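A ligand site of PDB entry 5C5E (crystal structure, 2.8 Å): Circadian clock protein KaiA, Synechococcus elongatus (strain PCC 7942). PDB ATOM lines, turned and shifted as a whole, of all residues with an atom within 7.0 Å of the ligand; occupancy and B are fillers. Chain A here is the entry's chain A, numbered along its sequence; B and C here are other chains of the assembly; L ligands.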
ATOM      1  N   ASN A 209       4.440  32.454 -17.880  1.00  0.00           N
ATOM      2  CA  ASN A 209       4.324  31.101 -17.341  1.00  0.00           C
ATOM      3  C   ASN A 209       2.872  30.687 -17.158  1.00  0.00           C
ATOM      4  O   ASN A 209       2.452  30.271 -16.078  1.00  0.00           O
ATOM      5  CB  ASN A 209       5.070  30.984 -16.010  1.00  0.00           C
ATOM      6  CG  ASN A 209       6.520  31.430 -16.113  1.00  0.00           C
ATOM      7  OD1 ASN A 209       7.159  31.244 -17.148  1.00  0.00           O
ATOM      8  ND2 ASN A 209       7.034  32.032 -15.051  1.00  0.00           N
ATOM      9  N   SER A 210       2.093  30.837 -18.228  1.00  0.00           N
ATOM     10  CA  SER A 210       0.681  30.537 -18.185  1.00  0.00           C
ATOM     11  C   SER A 210       0.279  29.657 -19.363  1.00  0.00           C
ATOM     12  O   SER A 210       1.104  29.276 -20.187  1.00  0.00           O
ATOM     13  CB  SER A 210      -0.144  31.822 -18.187  1.00  0.00           C
ATOM     14  OG  SER A 210      -1.522  31.540 -18.367  1.00  0.00           O
ATOM     15  N   ASN A 211      -1.007  29.353 -19.436  1.00  0.00           N
ATOM     16  CA  ASN A 211      -1.546  28.557 -20.527  1.00  0.00           C
ATOM     17  C   ASN A 211      -1.927  29.444 -21.702  1.00  0.00           C
ATOM     18  O   ASN A 211      -2.746  29.053 -22.539  1.00  0.00           O
ATOM     19  CB  ASN A 211      -2.746  27.734 -20.056  1.00  0.00           C
ATOM     20  CG  ASN A 211      -2.407  26.827 -18.886  1.00  0.00           C
ATOM     21  OD1 ASN A 211      -1.261  26.388 -18.728  1.00  0.00           O
ATOM     22  ND2 ASN A 211      -3.404  26.529 -18.055  1.00  0.00           N
ATOM     23  N   LEU A 212      -1.343  30.634 -21.743  1.00  0.00           N
ATOM     24  CA  LEU A 212      -1.604  31.613 -22.797  1.00  0.00           C
ATOM     25  C   LEU A 212      -1.502  30.998 -24.201  1.00  0.00           C
ATOM     26  O   LEU A 212      -2.417  31.129 -25.002  1.00  0.00           O
ATOM     27  CB  LEU A 212      -0.637  32.793 -22.688  1.00  0.00           C
ATOM     28  CG  LEU A 212      -0.697  33.779 -23.857  1.00  0.00           C
ATOM     29  CD1 LEU A 212      -2.076  34.435 -23.940  1.00  0.00           C
ATOM     30  CD2 LEU A 212       0.392  34.842 -23.731  1.00  0.00           C
ATOM     31  N   ASN A 213      -0.390  30.331 -24.468  1.00  0.00           N
ATOM     32  CA  ASN A 213      -0.171  29.710 -25.761  1.00  0.00           C
ATOM     33  C   ASN A 213      -1.114  28.538 -25.981  1.00  0.00           C
ATOM     34  O   ASN A 213      -1.551  28.281 -27.111  1.00  0.00           O
ATOM     35  CB  ASN A 213       1.279  29.246 -25.895  1.00  0.00           C
ATOM     36  CG  ASN A 213       2.273  30.314 -25.483  1.00  0.00           C
ATOM     37  OD1 ASN A 213       3.293  30.024 -24.845  1.00  0.00           O
ATOM     38  ND2 ASN A 213       2.008  31.549 -25.872  1.00  0.00           N
ATOM     39  N   GLN A 214      -1.442  27.824 -24.909  1.00  0.00           N
ATOM     40  CA  GLN A 214      -2.417  26.740 -24.986  1.00  0.00           C
ATOM     41  C   GLN A 214      -3.813  27.329 -25.184  1.00  0.00           C
ATOM     42  O   GLN A 214      -4.678  26.709 -25.799  1.00  0.00           O
ATOM     43  CB  GLN A 214      -2.375  25.869 -23.725  1.00  0.00           C
ATOM     44  CG  GLN A 214      -1.065  25.126 -23.519  1.00  0.00           C
ATOM     45  CD  GLN A 214      -0.826  24.054 -24.578  1.00  0.00           C
ATOM     46  OE1 GLN A 214      -1.355  22.954 -24.492  1.00  0.00           O
ATOM     47  NE2 GLN A 214      -0.009  24.392 -25.584  1.00  0.00           N
ATOM     48  N   SER A 215      -4.020  28.531 -24.673  1.00  0.00           N
ATOM     49  CA  SER A 215      -5.285  29.236 -24.851  1.00  0.00           C
ATOM     50  C   SER A 215      -5.422  29.750 -26.276  1.00  0.00           C
ATOM     51  O   SER A 215      -6.511  29.756 -26.841  1.00  0.00           O
ATOM     52  CB  SER A 215      -5.402  30.406 -23.856  1.00  0.00           C
ATOM     53  OG  SER A 215      -5.433  29.939 -22.526  1.00  0.00           O
ATOM     54  N   ILE A 216      -4.297  30.182 -26.850  1.00  0.00           N
ATOM     55  CA  ILE A 216      -4.275  30.651 -28.225  1.00  0.00           C
ATOM     56  C   ILE A 216      -4.574  29.516 -29.188  1.00  0.00           C
ATOM     57  O   ILE A 216      -5.409  29.653 -30.082  1.00  0.00           O
ATOM     58  CB  ILE A 216      -2.912  31.283 -28.583  1.00  0.00           C
ATOM     59  CG1 ILE A 216      -2.726  32.610 -27.840  1.00  0.00           C
ATOM     60  CG2 ILE A 216      -2.787  31.497 -30.080  1.00  0.00           C
ATOM     61  CD1 ILE A 216      -1.410  33.294 -28.134  1.00  0.00           C
ATOM     62  N   ASP A 217      -3.901  28.388 -28.995  1.00  0.00           N
ATOM     63  CA  ASP A 217      -4.097  27.204 -29.821  1.00  0.00           C
ATOM     64  C   ASP A 217      -5.550  26.784 -29.872  1.00  0.00           C
ATOM     65  O   ASP A 217      -6.087  26.508 -30.944  1.00  0.00           O
ATOM     66  CB  ASP A 217      -3.247  26.042 -29.307  1.00  0.00           C
ATOM     67  CG  ASP A 217      -1.762  26.299 -29.438  1.00  0.00           C
ATOM     68  OD1 ASP A 217      -1.380  27.143 -30.270  1.00  0.00           O
ATOM     69  OD2 ASP A 217      -0.980  25.650 -28.716  1.00  0.00           O
ATOM     70  N   HIS A 271      -0.612  32.994 -35.435  1.00  0.00           N
ATOM     71  CA  HIS A 271      -0.857  31.569 -35.244  1.00  0.00           C
ATOM     72  C   HIS A 271      -1.797  31.029 -36.304  1.00  0.00           C
ATOM     73  O   HIS A 271      -1.532  29.998 -36.917  1.00  0.00           O
ATOM     74  CB  HIS A 271      -1.444  31.313 -33.857  1.00  0.00           C
ATOM     75  CG  HIS A 271      -0.430  31.318 -32.750  1.00  0.00           C
ATOM     76  ND1 HIS A 271       0.168  32.470 -32.295  1.00  0.00           N
ATOM     77  CD2 HIS A 271       0.084  30.299 -32.023  1.00  0.00           C
ATOM     78  CE1 HIS A 271       1.016  32.164 -31.333  1.00  0.00           C
ATOM     79  NE2 HIS A 271       0.986  30.859 -31.139  1.00  0.00           N
ATOM     80  N   ILE B   9       8.327  38.488 -28.911  1.00  0.00           N
ATOM     81  CA  ILE B   9       7.346  37.699 -28.180  1.00  0.00           C
ATOM     82  C   ILE B   9       6.477  36.913 -29.154  1.00  0.00           C
ATOM     83  O   ILE B   9       6.309  35.698 -29.016  1.00  0.00           O
ATOM     84  CB  ILE B   9       6.445  38.578 -27.298  1.00  0.00           C
ATOM     85  CG1 ILE B   9       7.294  39.422 -26.334  1.00  0.00           C
ATOM     86  CG2 ILE B   9       5.418  37.731 -26.554  1.00  0.00           C
ATOM     87  CD1 ILE B   9       8.310  38.635 -25.546  1.00  0.00           C
ATOM     88  N   GLY B  12       8.730  34.107 -31.465  1.00  0.00           N
ATOM     89  CA  GLY B  12       9.093  32.797 -30.961  1.00  0.00           C
ATOM     90  C   GLY B  12       7.937  31.892 -30.590  1.00  0.00           C
ATOM     91  O   GLY B  12       8.094  30.666 -30.540  1.00  0.00           O
ATOM     92  N   VAL B  13       6.774  32.478 -30.319  1.00  0.00           N
ATOM     93  CA  VAL B  13       5.626  31.716 -29.840  1.00  0.00           C
ATOM     94  C   VAL B  13       5.017  30.825 -30.924  1.00  0.00           C
ATOM     95  O   VAL B  13       4.558  29.721 -30.650  1.00  0.00           O
ATOM     96  CB  VAL B  13       4.530  32.651 -29.264  1.00  0.00           C
ATOM     97  CG1 VAL B  13       4.100  33.674 -30.295  1.00  0.00           C
ATOM     98  CG2 VAL B  13       3.332  31.844 -28.768  1.00  0.00           C
ATOM     99  N   GLN B  14       5.031  31.295 -32.175  1.00  0.00           N
ATOM    100  CA  GLN B  14       4.422  30.543 -33.261  1.00  0.00           C
ATOM    101  C   GLN B  14       5.464  29.727 -34.027  1.00  0.00           C
ATOM    102  O   GLN B  14       5.396  29.597 -35.244  1.00  0.00           O
ATOM    103  CB  GLN B  14       3.687  31.485 -34.207  1.00  0.00           C
ATOM    104  CG  GLN B  14       4.543  32.615 -34.759  1.00  0.00           C
ATOM    105  CD  GLN B  14       3.968  33.191 -36.029  1.00  0.00           C
ATOM    106  OE1 GLN B  14       2.952  32.720 -36.533  1.00  0.00           O
ATOM    107  NE2 GLN B  14       4.626  34.225 -36.560  1.00  0.00           N
ATOM    108  N   GLU B  15       6.425  29.181 -33.286  1.00  0.00           N
ATOM    109  CA  GLU B  15       7.487  28.361 -33.874  1.00  0.00           C
ATOM    110  C   GLU B  15       7.393  26.815 -33.729  1.00  0.00           C
ATOM    111  O   GLU B  15       7.790  26.126 -34.663  1.00  0.00           O
ATOM    112  CB  GLU B  15       8.832  28.827 -33.306  1.00  0.00           C
ATOM    113  CG  GLU B  15       9.267  30.181 -33.849  1.00  0.00           C
ATOM    114  CD  GLU B  15      10.767  30.377 -33.822  1.00  0.00           C
ATOM    115  OE1 GLU B  15      11.354  30.358 -32.711  1.00  0.00           O
ATOM    116  OE2 GLU B  15      11.362  30.536 -34.903  1.00  0.00           O
ATOM    117  N   LYS B  16       6.900  26.245 -32.625  1.00  0.00           N
ATOM    118  CA  LYS B  16       6.324  26.927 -31.465  1.00  0.00           C
ATOM    119  C   LYS B  16       6.999  26.488 -30.175  1.00  0.00           C
ATOM    120  O   LYS B  16       7.047  27.240 -29.196  1.00  0.00           O
ATOM    121  CB  LYS B  16       4.818  26.672 -31.395  1.00  0.00           C
ATOM    122  CG  LYS B  16       4.096  26.912 -32.721  1.00  0.00           C
ATOM    123  CD  LYS B  16       2.579  26.993 -32.568  1.00  0.00           C
ATOM    124  CE  LYS B  16       1.928  27.360 -33.902  1.00  0.00           C
ATOM    125  NZ  LYS B  16       0.444  27.532 -33.816  1.00  0.00           N
ATOM    126  N   ALA C  94      -3.623  21.016 -18.912  1.00  0.00           N
ATOM    127  CA  ALA C  94      -2.304  20.466 -18.611  1.00  0.00           C
ATOM    128  C   ALA C  94      -1.186  21.376 -19.132  1.00  0.00           C
ATOM    129  O   ALA C  94      -1.389  22.168 -20.050  1.00  0.00           O
ATOM    130  CB  ALA C  94      -2.160  19.070 -19.198  1.00  0.00           C
ATOM    131  N   LYS C  95       0.001  21.250 -18.544  1.00  0.00           N
ATOM    132  CA  LYS C  95       1.110  22.139 -18.862  1.00  0.00           C
ATOM    133  C   LYS C  95       2.211  21.461 -19.691  1.00  0.00           C
ATOM    134  O   LYS C  95       2.642  22.008 -20.704  1.00  0.00           O
ATOM    135  CB  LYS C  95       1.714  22.719 -17.575  1.00  0.00           C
ATOM    136  CG  LYS C  95       0.779  23.694 -16.861  1.00  0.00           C
ATOM    137  CD  LYS C  95       1.371  24.205 -15.563  1.00  0.00           C
ATOM    138  CE  LYS C  95       1.447  23.109 -14.511  1.00  0.00           C
ATOM    139  NZ  LYS C  95       1.972  23.619 -13.210  1.00  0.00           N
ATOM    140  N   GLU C  96       2.664  20.287 -19.263  1.00  0.00           N
ATOM    141  CA  GLU C  96       3.685  19.567 -20.013  1.00  0.00           C
ATOM    142  C   GLU C  96       3.067  18.432 -20.841  1.00  0.00           C
ATOM    143  O   GLU C  96       1.926  18.029 -20.591  1.00  0.00           O
ATOM    144  CB  GLU C  96       4.764  19.001 -19.084  1.00  0.00           C
ATOM    145  CG  GLU C  96       4.334  17.744 -18.325  1.00  0.00           C
ATOM    146  CD  GLU C  96       5.513  16.873 -17.930  1.00  0.00           C
ATOM    147  OE1 GLU C  96       5.294  15.822 -17.296  1.00  0.00           O
ATOM    148  OE2 GLU C  96       6.662  17.245 -18.251  1.00  0.00           O
ATOM    149  N   GLN C  97       3.816  17.938 -21.822  1.00  0.00           N
ATOM    150  CA  GLN C  97       3.364  16.820 -22.644  1.00  0.00           C
ATOM    151  C   GLN C  97       3.246  15.555 -21.806  1.00  0.00           C
ATOM    152  O   GLN C  97       4.201  15.138 -21.152  1.00  0.00           O
ATOM    153  CB  GLN C  97       4.318  16.593 -23.811  1.00  0.00           C
ATOM    154  CG  GLN C  97       4.911  17.872 -24.420  1.00  0.00           C
ATOM    155  CD  GLN C  97       4.224  18.293 -25.713  1.00  0.00           C
ATOM    156  OE1 GLN C  97       2.999  18.354 -25.801  1.00  0.00           O
ATOM    157  NE2 GLN C  97       5.027  18.599 -26.733  1.00  0.00           N
HETATM  158  S1  LIG L   1       6.159  22.381 -18.611  1.00  0.00           S
HETATM  159  C1  LIG L   1       5.763  23.645 -19.633  1.00  0.00           C
HETATM  160  N1  LIG L   1       6.029  23.501 -21.061  1.00  0.00           N
HETATM  161  C2  LIG L   1       5.745  24.530 -22.071  1.00  0.00           C
HETATM  162  C3  LIG L   1       4.687  25.445 -21.942  1.00  0.00           C
HETATM  163  C4  LIG L   1       4.458  26.409 -22.931  1.00  0.00           C
HETATM  164  C5  LIG L   1       3.289  27.400 -22.763  1.00  0.00           C
HETATM  165  O1  LIG L   1       3.504  28.617 -22.459  1.00  0.00           O
HETATM  166  O2  LIG L   1       2.090  27.014 -22.933  1.00  0.00           O
HETATM  167  C6  LIG L   1       6.557  24.591 -23.200  1.00  0.00           C
HETATM  168  C7  LIG L   1       6.332  25.542 -24.192  1.00  0.00           C
HETATM  169  C8  LIG L   1       5.290  26.463 -24.064  1.00  0.00           C
HETATM  170  C9  LIG L   1       5.062  27.439 -25.093  1.00  0.00           C
HETATM  171  C10 LIG L   1       6.028  28.468 -25.112  1.00  0.00           C
HETATM  172  C11 LIG L   1       6.127  29.306 -26.216  1.00  0.00           C
HETATM  173  O3  LIG L   1       5.261  29.141 -27.315  1.00  0.00           O
HETATM  174  C12 LIG L   1       7.083  30.344 -26.253  1.00  0.00           C
HETATM  175  C13 LIG L   1       6.898  28.670 -24.030  1.00  0.00           C
HETATM  176  C14 LIG L   1       7.862  29.686 -24.060  1.00  0.00           C
HETATM  177  C15 LIG L   1       7.948  30.527 -25.166  1.00  0.00           C
HETATM  178  O4  LIG L   1       8.774  31.412 -25.198  1.00  0.00           O
HETATM  179  C16 LIG L   1       4.193  27.284 -26.202  1.00  0.00           C
HETATM  180  C17 LIG L   1       4.301  28.130 -27.301  1.00  0.00           C
HETATM  181  C18 LIG L   1       3.435  27.966 -28.400  1.00  0.00           C
HETATM  182  C19 LIG L   1       3.230  26.260 -26.199  1.00  0.00           C
HETATM  183  C20 LIG L   1       2.371  26.095 -27.291  1.00  0.00           C
HETATM  184  C21 LIG L   1       2.482  26.951 -28.392  1.00  0.00           C
HETATM  185  O5  LIG L   1       1.638  26.826 -29.523  1.00  0.00           O
HETATM  186  O6  LIG L   1       5.159  24.831 -19.052  1.00  0.00           O
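An oxygen (O5) of the ligand sits at hydrogen-bond distance from the side-chain carboxylate (OD2) of Asp 217, at 3.0 Å. The side-chain amide oxygen of Asn 213 sits close to an oxygen (O1) of the ligand (2.8 Å).
An oxygen (O1) of the ligand lies close to the backbone carbonyl oxygen (O) of Ser 210 (3.4 Å). An oxygen (O3) of the ligand lies close to the backbone carbonyl oxygen (O) of Val 13 of chain B, at 3.5 Å. O of Lys 16 of chain B lies close to O3 of the ligand, at 3.2 Å. Gln 214 touches the ligand (NE2 to C20, 3.4 Å). Lys 95 of chain C touches the ligand (O to C1, 3.7 Å). Glu 96 of chain C touches the ligand. Hydrophobic or aromatic side chains within 4 Å of the ligand: Val 13 of chain B. Eight residues have an atom within 4 Å of the ligand: Ser 210, Asn 213, Gln 214, Asp 217, Val 13 of chain B, Lys 16 of chain B, Lys 95 of chain C and Glu 96 of chain C. The nearest printed residue that does not touch the ligand is His 271 (4.4 Å).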
